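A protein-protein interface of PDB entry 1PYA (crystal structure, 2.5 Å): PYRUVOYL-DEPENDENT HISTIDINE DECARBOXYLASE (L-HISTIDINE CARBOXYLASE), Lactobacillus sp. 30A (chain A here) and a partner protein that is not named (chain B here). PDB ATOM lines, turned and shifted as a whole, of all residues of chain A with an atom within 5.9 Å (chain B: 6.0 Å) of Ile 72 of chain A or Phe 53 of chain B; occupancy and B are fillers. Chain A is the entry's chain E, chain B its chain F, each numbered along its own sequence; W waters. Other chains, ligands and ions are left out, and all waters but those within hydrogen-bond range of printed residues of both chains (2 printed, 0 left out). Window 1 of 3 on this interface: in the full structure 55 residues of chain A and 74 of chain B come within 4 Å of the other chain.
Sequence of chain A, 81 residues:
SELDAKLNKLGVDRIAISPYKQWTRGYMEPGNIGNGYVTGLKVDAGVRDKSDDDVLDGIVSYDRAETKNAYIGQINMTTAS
N of Thr 24 of chain A is in hydrogen-bond range of O of Tyr 62 of chain B, 3.0 Å away.
The backbone carbonyl oxygen (O) of Lys 42 of chain A sits at hydrogen-bond distance from the backbone NH (N) of Val 178 of chain B (2.8 Å).
O of His 61 of chain B is in hydrogen-bond range of OG1 of Thr 24 of chain A (2.9 Å).
The side-chain hydroxyl (OG1) of Thr 24 of chain A sits close to the backbone nitrogen (N) of Pro 63 of chain B (3.1 Å).
The backbone NH (N) of Tyr 71 of chain A sits at hydrogen-bond distance from the backbone carbonyl oxygen (O) of Gly 54 of chain B, 2.9 Å away.
The backbone NH (N) of Ile 72 of chain A is in hydrogen-bond range of the backbone carbonyl oxygen (O) of Glu 66 of chain A (3.0 Å).
NZ of Lys 42 of chain A sits at hydrogen-bond distance from O of Ala 70 of chain A, 2.9 Å away.
The backbone carbonyl oxygen (O) of Phe 53 of chain B sits at hydrogen-bond distance from the backbone NH (N) of Arg 60 of chain B (2.9 Å).
O of Tyr 52 of chain B is in hydrogen-bond range of N of His 61 of chain B (2.9 Å).
The side-chain amino group (NZ) of Lys 42 of chain A lies within hydrogen-bond range of the backbone carbonyl oxygen (O) of Ala 65 of chain A (3.0 Å).
The side-chain hydroxyl (OG1) of Thr 55 of chain B is in hydrogen-bond range of the backbone NH (N) of Asp 58 of chain B.
Among the printed residues, merely in contact across the chains: Tyr 71 of chain A with Tyr 62 of chain B, Ile 72 of chain A with Phe 53 of chain B, Ala 70 of chain A with Gly 54 of chain B, Met 77 of chain A with Cys 71 of chain B, Ile 75 of chain A with Pro 63 of chain B, Tyr 71 of chain A with Arg 59 of chain B, Tyr 71 of chain A with Pro 63 of chain B, Tyr 71 of chain A with Thr 55 of chain B, Tyr 71 of chain A with Phe 53 of chain B, Thr 24 of chain A with Phe 53 of chain B, Thr 24 of chain A with Tyr 52 of chain B, Ala 70 of chain A with Val 50 of chain B and Ala 65 of chain A with Ile 176 of chain B.
Ile 72 of chain A touches just one residue of chain B: Phe 53.
Phe 53 of chain B touches just these residues of chain A: Thr 24, Tyr 71 and Ile 72.
Of the printed residues of chain A, Arg 59 of chain B touches Tyr 71 (3.6 Å).
Of the printed residues of chain A, Val 178 of chain B touches Lys 42.
Of the printed residues of chain A, Val 50 of chain B touches Ala 70 (3.8 Å).
Ala 48 of chain B touches none of the printed residues of chain A.
The nearest printed residue of chain A that does not touch Ile 176 of chain B is Lys 42 of chain A (4.2 Å).
Along chain A the printed residues that touch a printed residue of chain B span positions 24 to 77.
Of the 20 printed residues of chain B, 12 touch a printed residue of chain A.
Hydrophobic or aromatic side chains of chain B within 4 Å of the printed part of chain A: Val 50, Tyr 52, Phe 53, Tyr 62, Pro 63, Ile 176 and Val 178.
Among the printed residues, 18 pairs touch across the chains.
Among the printed residues, no Asp or Glu carboxylate lies within 4 Å of a Lys or Arg side-chain nitrogen of the other chain.
Water W1 bridges NH2 of Arg 59 of chain B (2.7 Å) and OE1 of Gln 74 of chain A (3.1 Å).
Water W2 bridges the backbone carbonyl oxygen (O) of Pro 63 of chain B (2.8 Å) and the backbone carbonyl oxygen (O) of Gly 73 of chain A (3.0 Å).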
ATOM      1  N   THR A  24       8.661   0.042 -18.649  1.00  0.00           N
ATOM      2  CA  THR A  24       9.821  -0.774 -18.439  1.00  0.00           C
ATOM      3  C   THR A  24       9.455  -1.781 -17.334  1.00  0.00           C
ATOM      4  O   THR A  24       8.478  -1.627 -16.596  1.00  0.00           O
ATOM      5  CB  THR A  24      11.075   0.073 -17.999  1.00  0.00           C
ATOM      6  OG1 THR A  24      10.662   1.129 -17.138  1.00  0.00           O
ATOM      7  CG2 THR A  24      11.794   0.701 -19.200  1.00  0.00           C
ATOM      8  N   LYS A  42      20.017   7.422 -10.695  1.00  0.00           N
ATOM      9  CA  LYS A  42      19.040   8.276 -10.039  1.00  0.00           C
ATOM     10  C   LYS A  42      19.531   8.608  -8.645  1.00  0.00           C
ATOM     11  O   LYS A  42      19.818   7.701  -7.858  1.00  0.00           O
ATOM     12  CB  LYS A  42      17.657   7.583  -9.921  1.00  0.00           C
ATOM     13  CG  LYS A  42      16.645   8.441  -9.184  1.00  0.00           C
ATOM     14  CD  LYS A  42      15.231   7.878  -9.101  1.00  0.00           C
ATOM     15  CE  LYS A  42      14.537   8.723  -8.037  1.00  0.00           C
ATOM     16  NZ  LYS A  42      13.643   9.759  -8.535  1.00  0.00           N
ATOM     17  N   ALA A  65      11.147  11.068  -2.696  1.00  0.00           N
ATOM     18  CA  ALA A  65      12.378  10.990  -3.454  1.00  0.00           C
ATOM     19  C   ALA A  65      12.171  10.134  -4.716  1.00  0.00           C
ATOM     20  O   ALA A  65      12.669  10.489  -5.783  1.00  0.00           O
ATOM     21  CB  ALA A  65      13.475  10.365  -2.575  1.00  0.00           C
ATOM     22  N   GLU A  66      11.433   9.020  -4.671  1.00  0.00           N
ATOM     23  CA  GLU A  66      11.166   8.171  -5.846  1.00  0.00           C
ATOM     24  C   GLU A  66      10.343   8.810  -6.962  1.00  0.00           C
ATOM     25  O   GLU A  66      10.380   8.425  -8.139  1.00  0.00           O
ATOM     26  CB  GLU A  66      10.426   6.909  -5.436  1.00  0.00           C
ATOM     27  CG  GLU A  66      11.190   5.917  -4.620  1.00  0.00           C
ATOM     28  CD  GLU A  66      10.426   4.626  -4.313  1.00  0.00           C
ATOM     29  OE1 GLU A  66       9.278   4.671  -3.869  1.00  0.00           O
ATOM     30  OE2 GLU A  66      10.978   3.546  -4.518  1.00  0.00           O
ATOM     31  N   THR A  67       9.513   9.747  -6.532  1.00  0.00           N
ATOM     32  CA  THR A  67       8.533  10.474  -7.303  1.00  0.00           C
ATOM     33  C   THR A  67       9.040  11.756  -7.922  1.00  0.00           C
ATOM     34  O   THR A  67       8.444  12.292  -8.852  1.00  0.00           O
ATOM     35  CB  THR A  67       7.427  10.589  -6.242  1.00  0.00           C
ATOM     36  OG1 THR A  67       6.505   9.588  -6.679  1.00  0.00           O
ATOM     37  CG2 THR A  67       6.864  11.960  -5.984  1.00  0.00           C
ATOM     38  N   ALA A  70      13.299  11.640 -12.175  1.00  0.00           N
ATOM     39  CA  ALA A  70      13.019  10.477 -13.009  1.00  0.00           C
ATOM     40  C   ALA A  70      12.022   9.671 -12.213  1.00  0.00           C
ATOM     41  O   ALA A  70      12.302   9.233 -11.099  1.00  0.00           O
ATOM     42  CB  ALA A  70      14.284   9.609 -13.255  1.00  0.00           C
ATOM     43  N   TYR A  71      10.838   9.490 -12.765  1.00  0.00           N
ATOM     44  CA  TYR A  71       9.786   8.772 -12.078  1.00  0.00           C
ATOM     45  C   TYR A  71       9.971   7.275 -11.915  1.00  0.00           C
ATOM     46  O   TYR A  71       9.863   6.529 -12.895  1.00  0.00           O
ATOM     47  CB  TYR A  71       8.433   9.027 -12.786  1.00  0.00           C
ATOM     48  CG  TYR A  71       7.225   8.497 -12.020  1.00  0.00           C
ATOM     49  CD1 TYR A  71       6.771   9.115 -10.864  1.00  0.00           C
ATOM     50  CD2 TYR A  71       6.554   7.398 -12.508  1.00  0.00           C
ATOM     51  CE1 TYR A  71       5.663   8.624 -10.214  1.00  0.00           C
ATOM     52  CE2 TYR A  71       5.438   6.899 -11.866  1.00  0.00           C
ATOM     53  CZ  TYR A  71       5.007   7.518 -10.719  1.00  0.00           C
ATOM     54  OH  TYR A  71       3.908   6.990 -10.084  1.00  0.00           O
ATOM     55  N   ILE A  72      10.191   6.833 -10.673  1.00  0.00           N
ATOM     56  CA  ILE A  72      10.184   5.411 -10.364  1.00  0.00           C
ATOM     57  C   ILE A  72       9.156   5.088  -9.265  1.00  0.00           C
ATOM     58  O   ILE A  72       9.302   4.138  -8.491  1.00  0.00           O
ATOM     59  CB  ILE A  72      11.555   4.855  -9.883  1.00  0.00           C
ATOM     60  CG1 ILE A  72      12.142   5.622  -8.721  1.00  0.00           C
ATOM     61  CG2 ILE A  72      12.491   4.884 -11.073  1.00  0.00           C
ATOM     62  CD1 ILE A  72      13.235   4.752  -8.030  1.00  0.00           C
ATOM     63  N   GLY A  73       8.092   5.867  -9.119  1.00  0.00           N
ATOM     64  CA  GLY A  73       7.058   5.583  -8.136  1.00  0.00           C
ATOM     65  C   GLY A  73       6.322   4.283  -8.443  1.00  0.00           C
ATOM     66  O   GLY A  73       6.307   3.777  -9.559  1.00  0.00           O
ATOM     67  N   GLN A  74       5.778   3.704  -7.374  1.00  0.00           N
ATOM     68  CA  GLN A  74       4.927   2.501  -7.351  1.00  0.00           C
ATOM     69  C   GLN A  74       5.548   1.210  -7.849  1.00  0.00           C
ATOM     70  O   GLN A  74       4.925   0.287  -8.421  1.00  0.00           O
ATOM     71  CB  GLN A  74       3.610   2.774  -8.126  1.00  0.00           C
ATOM     72  CG  GLN A  74       2.745   3.921  -7.560  1.00  0.00           C
ATOM     73  CD  GLN A  74       1.281   3.850  -8.012  1.00  0.00           C
ATOM     74  OE1 GLN A  74       0.896   3.570  -9.140  1.00  0.00           O
ATOM     75  NE2 GLN A  74       0.331   3.976  -7.116  1.00  0.00           N
ATOM     76  N   ILE A  75       6.821   1.084  -7.482  1.00  0.00           N
ATOM     77  CA  ILE A  75       7.586  -0.096  -7.811  1.00  0.00           C
ATOM     78  C   ILE A  75       7.976  -0.789  -6.527  1.00  0.00           C
ATOM     79  O   ILE A  75       8.077  -0.177  -5.473  1.00  0.00           O
ATOM     80  CB  ILE A  75       8.920   0.200  -8.590  1.00  0.00           C
ATOM     81  CG1 ILE A  75       9.900   1.011  -7.760  1.00  0.00           C
ATOM     82  CG2 ILE A  75       8.528   0.888  -9.894  1.00  0.00           C
ATOM     83  CD1 ILE A  75      11.323   0.932  -8.273  1.00  0.00           C
ATOM     84  N   MET A  77      11.000  -2.273  -4.857  1.00  0.00           N
ATOM     85  CA  MET A  77      12.431  -2.202  -5.045  1.00  0.00           C
ATOM     86  C   MET A  77      13.100  -3.292  -4.252  1.00  0.00           C
ATOM     87  O   MET A  77      12.821  -3.370  -3.057  1.00  0.00           O
ATOM     88  CB  MET A  77      12.935  -0.856  -4.578  1.00  0.00           C
ATOM     89  CG  MET A  77      14.385  -0.580  -4.959  1.00  0.00           C
ATOM     90  SD  MET A  77      15.084   0.926  -4.242  1.00  0.00           S
ATOM     91  CE  MET A  77      14.075   2.098  -5.120  1.00  0.00           C
ATOM     92  N   ILE B  10      21.939   3.771 -19.727  1.00  0.00           N
ATOM     93  CA  ILE B  10      21.201   4.806 -20.406  1.00  0.00           C
ATOM     94  C   ILE B  10      21.999   6.074 -20.342  1.00  0.00           C
ATOM     95  O   ILE B  10      22.532   6.468 -19.281  1.00  0.00           O
ATOM     96  CB  ILE B  10      19.817   4.995 -19.725  1.00  0.00           C
ATOM     97  CG1 ILE B  10      19.026   3.717 -19.919  1.00  0.00           C
ATOM     98  CG2 ILE B  10      19.045   6.162 -20.326  1.00  0.00           C
ATOM     99  CD1 ILE B  10      17.544   3.751 -19.415  1.00  0.00           C
ATOM    100  N   ALA B  48      19.768  11.922 -18.543  1.00  0.00           N
ATOM    101  CA  ALA B  48      19.287  11.012 -19.562  1.00  0.00           C
ATOM    102  C   ALA B  48      18.195  10.103 -19.001  1.00  0.00           C
ATOM    103  O   ALA B  48      17.177   9.863 -19.680  1.00  0.00           O
ATOM    104  CB  ALA B  48      20.451  10.178 -20.072  1.00  0.00           C
ATOM    105  N   LEU B  49      18.336   9.656 -17.742  1.00  0.00           N
ATOM    106  CA  LEU B  49      17.343   8.758 -17.176  1.00  0.00           C
ATOM    107  C   LEU B  49      16.016   9.474 -16.998  1.00  0.00           C
ATOM    108  O   LEU B  49      14.963   8.853 -17.217  1.00  0.00           O
ATOM    109  CB  LEU B  49      17.805   8.191 -15.829  1.00  0.00           C
ATOM    110  CG  LEU B  49      16.915   7.047 -15.285  1.00  0.00           C
ATOM    111  CD1 LEU B  49      17.075   5.834 -16.188  1.00  0.00           C
ATOM    112  CD2 LEU B  49      17.310   6.687 -13.834  1.00  0.00           C
ATOM    113  N   VAL B  50      15.978  10.769 -16.695  1.00  0.00           N
ATOM    114  CA  VAL B  50      14.685  11.400 -16.603  1.00  0.00           C
ATOM    115  C   VAL B  50      14.149  11.625 -18.011  1.00  0.00           C
ATOM    116  O   VAL B  50      12.921  11.552 -18.167  1.00  0.00           O
ATOM    117  CB  VAL B  50      14.730  12.742 -15.649  1.00  0.00           C
ATOM    118  CG1 VAL B  50      16.129  13.124 -15.251  1.00  0.00           C
ATOM    119  CG2 VAL B  50      13.972  13.874 -16.294  1.00  0.00           C
ATOM    120  N   GLU B  51      14.934  11.778 -19.086  1.00  0.00           N
ATOM    121  CA  GLU B  51      14.350  11.837 -20.433  1.00  0.00           C
ATOM    122  C   GLU B  51      13.632  10.530 -20.782  1.00  0.00           C
ATOM    123  O   GLU B  51      12.559  10.540 -21.386  1.00  0.00           O
ATOM    124  CB  GLU B  51      15.403  12.075 -21.542  1.00  0.00           C
ATOM    125  CG  GLU B  51      16.127  13.434 -21.550  1.00  0.00           C
ATOM    126  CD  GLU B  51      15.316  14.673 -21.894  1.00  0.00           C
ATOM    127  OE1 GLU B  51      14.088  14.609 -22.008  1.00  0.00           O
ATOM    128  OE2 GLU B  51      15.935  15.725 -22.050  1.00  0.00           O
ATOM    129  N   TYR B  52      14.217   9.401 -20.399  1.00  0.00           N
ATOM    130  CA  TYR B  52      13.657   8.109 -20.736  1.00  0.00           C
ATOM    131  C   TYR B  52      12.435   7.711 -19.909  1.00  0.00           C
ATOM    132  O   TYR B  52      11.403   7.257 -20.446  1.00  0.00           O
ATOM    133  CB  TYR B  52      14.779   7.089 -20.610  1.00  0.00           C
ATOM    134  CG  TYR B  52      14.368   5.763 -21.224  1.00  0.00           C
ATOM    135  CD1 TYR B  52      14.139   5.665 -22.592  1.00  0.00           C
ATOM    136  CD2 TYR B  52      14.133   4.693 -20.392  1.00  0.00           C
ATOM    137  CE1 TYR B  52      13.651   4.499 -23.145  1.00  0.00           C
ATOM    138  CE2 TYR B  52      13.645   3.519 -20.932  1.00  0.00           C
ATOM    139  CZ  TYR B  52      13.406   3.438 -22.294  1.00  0.00           C
ATOM    140  OH  TYR B  52      12.880   2.274 -22.787  1.00  0.00           O
ATOM    141  N   PHE B  53      12.539   7.814 -18.576  1.00  0.00           N
ATOM    142  CA  PHE B  53      11.447   7.450 -17.669  1.00  0.00           C
ATOM    143  C   PHE B  53      10.380   8.511 -17.621  1.00  0.00           C
ATOM    144  O   PHE B  53       9.208   8.191 -17.435  1.00  0.00           O
ATOM    145  CB  PHE B  53      11.935   7.224 -16.218  1.00  0.00           C
ATOM    146  CG  PHE B  53      12.596   5.884 -15.936  1.00  0.00           C
ATOM    147  CD1 PHE B  53      12.737   4.933 -16.930  1.00  0.00           C
ATOM    148  CD2 PHE B  53      13.062   5.638 -14.660  1.00  0.00           C
ATOM    149  CE1 PHE B  53      13.352   3.746 -16.617  1.00  0.00           C
ATOM    150  CE2 PHE B  53      13.678   4.447 -14.362  1.00  0.00           C
ATOM    151  CZ  PHE B  53      13.823   3.501 -15.340  1.00  0.00           C
ATOM    152  N   GLY B  54      10.744   9.744 -17.903  1.00  0.00           N
ATOM    153  CA  GLY B  54       9.798  10.835 -17.759  1.00  0.00           C
ATOM    154  C   GLY B  54       9.721  11.231 -16.287  1.00  0.00           C
ATOM    155  O   GLY B  54      10.417  10.642 -15.444  1.00  0.00           O
ATOM    156  N   THR B  55       8.938  12.238 -15.944  1.00  0.00           N
ATOM    157  CA  THR B  55       8.806  12.658 -14.579  1.00  0.00           C
ATOM    158  C   THR B  55       7.369  12.308 -14.186  1.00  0.00           C
ATOM    159  O   THR B  55       6.600  11.786 -15.029  1.00  0.00           O
ATOM    160  CB  THR B  55       9.080  14.152 -14.467  1.00  0.00           C
ATOM    161  OG1 THR B  55       8.142  14.791 -15.317  1.00  0.00           O
ATOM    162  CG2 THR B  55      10.485  14.566 -14.900  1.00  0.00           C
ATOM    163  N   ASP B  58       5.084  14.048 -16.455  1.00  0.00           N
ATOM    164  CA  ASP B  58       5.225  13.844 -17.883  1.00  0.00           C
ATOM    165  C   ASP B  58       5.813  12.475 -18.020  1.00  0.00           C
ATOM    166  O   ASP B  58       7.008  12.340 -18.238  1.00  0.00           O
ATOM    167  CB  ASP B  58       6.137  14.939 -18.372  1.00  0.00           C
ATOM    168  CG  ASP B  58       6.211  15.097 -19.874  1.00  0.00           C
ATOM    169  OD1 ASP B  58       5.613  14.307 -20.611  1.00  0.00           O
ATOM    170  OD2 ASP B  58       6.891  16.032 -20.300  1.00  0.00           O
ATOM    171  N   ARG B  59       4.971  11.471 -17.852  1.00  0.00           N
ATOM    172  CA  ARG B  59       5.462  10.129 -17.656  1.00  0.00           C
ATOM    173  C   ARG B  59       5.813   9.542 -19.004  1.00  0.00           C
ATOM    174  O   ARG B  59       5.059   9.722 -19.935  1.00  0.00           O
ATOM    175  CB  ARG B  59       4.393   9.263 -16.965  1.00  0.00           C
ATOM    176  CG  ARG B  59       3.664   9.972 -15.853  1.00  0.00           C
ATOM    177  CD  ARG B  59       3.846   9.476 -14.457  1.00  0.00           C
ATOM    178  NE  ARG B  59       2.761   8.610 -14.051  1.00  0.00           N
ATOM    179  CZ  ARG B  59       2.173   8.691 -12.843  1.00  0.00           C
ATOM    180  NH1 ARG B  59       2.367   9.715 -12.011  1.00  0.00           N
ATOM    181  NH2 ARG B  59       1.302   7.751 -12.486  1.00  0.00           N
ATOM    182  N   ARG B  60       6.930   8.841 -19.161  1.00  0.00           N
ATOM    183  CA  ARG B  60       7.330   8.284 -20.437  1.00  0.00           C
ATOM    184  C   ARG B  60       7.512   6.775 -20.215  1.00  0.00           C
ATOM    185  O   ARG B  60       6.554   6.086 -19.905  1.00  0.00           O
ATOM    186  CB  ARG B  60       8.642   8.982 -20.862  1.00  0.00           C
ATOM    187  CG  ARG B  60       8.560  10.012 -21.949  1.00  0.00           C
ATOM    188  CD  ARG B  60       8.608  11.481 -21.621  1.00  0.00           C
ATOM    189  NE  ARG B  60       9.935  11.961 -21.919  1.00  0.00           N
ATOM    190  CZ  ARG B  60      10.242  13.181 -22.382  1.00  0.00           C
ATOM    191  NH1 ARG B  60       9.345  14.092 -22.738  1.00  0.00           N
ATOM    192  NH2 ARG B  60      11.536  13.455 -22.532  1.00  0.00           N
ATOM    193  N   HIS B  61       8.695   6.139 -20.291  1.00  0.00           N
ATOM    194  CA  HIS B  61       8.778   4.683 -20.240  1.00  0.00           C
ATOM    195  C   HIS B  61       9.204   4.233 -18.859  1.00  0.00           C
ATOM    196  O   HIS B  61      10.180   3.506 -18.647  1.00  0.00           O
ATOM    197  CB  HIS B  61       9.750   4.241 -21.336  1.00  0.00           C
ATOM    198  CG  HIS B  61       9.172   4.683 -22.675  1.00  0.00           C
ATOM    199  ND1 HIS B  61       8.059   4.228 -23.253  1.00  0.00           N
ATOM    200  CD2 HIS B  61       9.632   5.720 -23.467  1.00  0.00           C
ATOM    201  CE1 HIS B  61       7.822   4.926 -24.336  1.00  0.00           C
ATOM    202  NE2 HIS B  61       8.771   5.831 -24.453  1.00  0.00           N
ATOM    203  N   TYR B  62       8.433   4.691 -17.883  1.00  0.00           N
ATOM    204  CA  TYR B  62       8.740   4.394 -16.472  1.00  0.00           C
ATOM    205  C   TYR B  62       8.368   2.959 -16.123  1.00  0.00           C
ATOM    206  O   TYR B  62       7.668   2.291 -16.909  1.00  0.00           O
ATOM    207  CB  TYR B  62       7.979   5.414 -15.530  1.00  0.00           C
ATOM    208  CG  TYR B  62       6.460   5.313 -15.587  1.00  0.00           C
ATOM    209  CD1 TYR B  62       5.790   5.909 -16.607  1.00  0.00           C
ATOM    210  CD2 TYR B  62       5.774   4.607 -14.629  1.00  0.00           C
ATOM    211  CE1 TYR B  62       4.429   5.790 -16.689  1.00  0.00           C
ATOM    212  CE2 TYR B  62       4.402   4.483 -14.700  1.00  0.00           C
ATOM    213  CZ  TYR B  62       3.752   5.074 -15.741  1.00  0.00           C
ATOM    214  OH  TYR B  62       2.401   4.948 -15.855  1.00  0.00           O
ATOM    215  N   PRO B  63       8.831   2.429 -14.990  1.00  0.00           N
ATOM    216  CA  PRO B  63       8.574   1.044 -14.608  1.00  0.00           C
ATOM    217  C   PRO B  63       7.077   0.774 -14.397  1.00  0.00           C
ATOM    218  O   PRO B  63       6.344   1.650 -13.933  1.00  0.00           O
ATOM    219  CB  PRO B  63       9.464   0.881 -13.364  1.00  0.00           C
ATOM    220  CG  PRO B  63      10.590   1.890 -13.476  1.00  0.00           C
ATOM    221  CD  PRO B  63       9.802   3.057 -14.079  1.00  0.00           C
ATOM    222  N   CYS B  71      17.533  -2.913  -7.715  1.00  0.00           N
ATOM    223  CA  CYS B  71      18.282  -1.695  -7.718  1.00  0.00           C
ATOM    224  C   CYS B  71      19.509  -1.777  -6.860  1.00  0.00           C
ATOM    225  O   CYS B  71      19.479  -2.378  -5.785  1.00  0.00           O
ATOM    226  CB  CYS B  71      17.481  -0.533  -7.174  1.00  0.00           C
ATOM    227  SG  CYS B  71      16.004  -0.151  -8.125  1.00  0.00           S
ATOM    228  N   ILE B 176      18.309   9.437  -1.472  1.00  0.00           N
ATOM    229  CA  ILE B 176      18.459   8.079  -1.992  1.00  0.00           C
ATOM    230  C   ILE B 176      19.331   8.087  -3.234  1.00  0.00           C
ATOM    231  O   ILE B 176      19.437   9.100  -3.928  1.00  0.00           O
ATOM    232  CB  ILE B 176      17.036   7.415  -2.318  1.00  0.00           C
ATOM    233  CG1 ILE B 176      16.385   7.960  -3.599  1.00  0.00           C
ATOM    234  CG2 ILE B 176      16.137   7.639  -1.080  1.00  0.00           C
ATOM    235  CD1 ILE B 176      15.210   7.076  -4.077  1.00  0.00           C
ATOM    236  N   VAL B 178      20.060   5.349  -6.380  1.00  0.00           N
ATOM    237  CA  VAL B 178      19.551   4.151  -7.034  1.00  0.00           C
ATOM    238  C   VAL B 178      19.893   4.000  -8.517  1.00  0.00           C
ATOM    239  O   VAL B 178      19.869   4.930  -9.336  1.00  0.00           O
ATOM    240  CB  VAL B 178      17.947   4.032  -6.742  1.00  0.00           C
ATOM    241  CG1 VAL B 178      17.299   5.349  -6.561  1.00  0.00           C
ATOM    242  CG2 VAL B 178      17.189   3.436  -7.890  1.00  0.00           C
ATOM    243  N   PRO B 180      18.580   1.347 -11.151  1.00  0.00           N
ATOM    244  CA  PRO B 180      17.616   0.321 -11.509  1.00  0.00           C
ATOM    245  C   PRO B 180      18.109  -0.641 -12.589  1.00  0.00           C
ATOM    246  O   PRO B 180      18.882  -0.208 -13.451  1.00  0.00           O
ATOM    247  CB  PRO B 180      16.392   1.068 -11.983  1.00  0.00           C
ATOM    248  CG  PRO B 180      16.763   2.531 -11.914  1.00  0.00           C
ATOM    249  CD  PRO B 180      18.280   2.598 -11.813  1.00  0.00           C
ATOM    250  N   VAL B 182      16.614  -2.709 -15.656  1.00  0.00           N
ATOM    251  CA  VAL B 182      15.384  -2.804 -16.432  1.00  0.00           C
ATOM    252  C   VAL B 182      15.427  -3.464 -17.826  1.00  0.00           C
ATOM    253  O   VAL B 182      16.500  -3.716 -18.381  1.00  0.00           O
ATOM    254  CB  VAL B 182      14.773  -1.337 -16.582  1.00  0.00           C
ATOM    255  CG1 VAL B 182      14.486  -0.705 -15.211  1.00  0.00           C
ATOM    256  CG2 VAL B 182      15.725  -0.477 -17.413  1.00  0.00           C
HETATM  257  O   HOH W   1       0.184   6.293 -10.465  1.00  0.00           O
HETATM  258  O   HOH W   2       4.782   2.539 -11.797  1.00  0.00           O
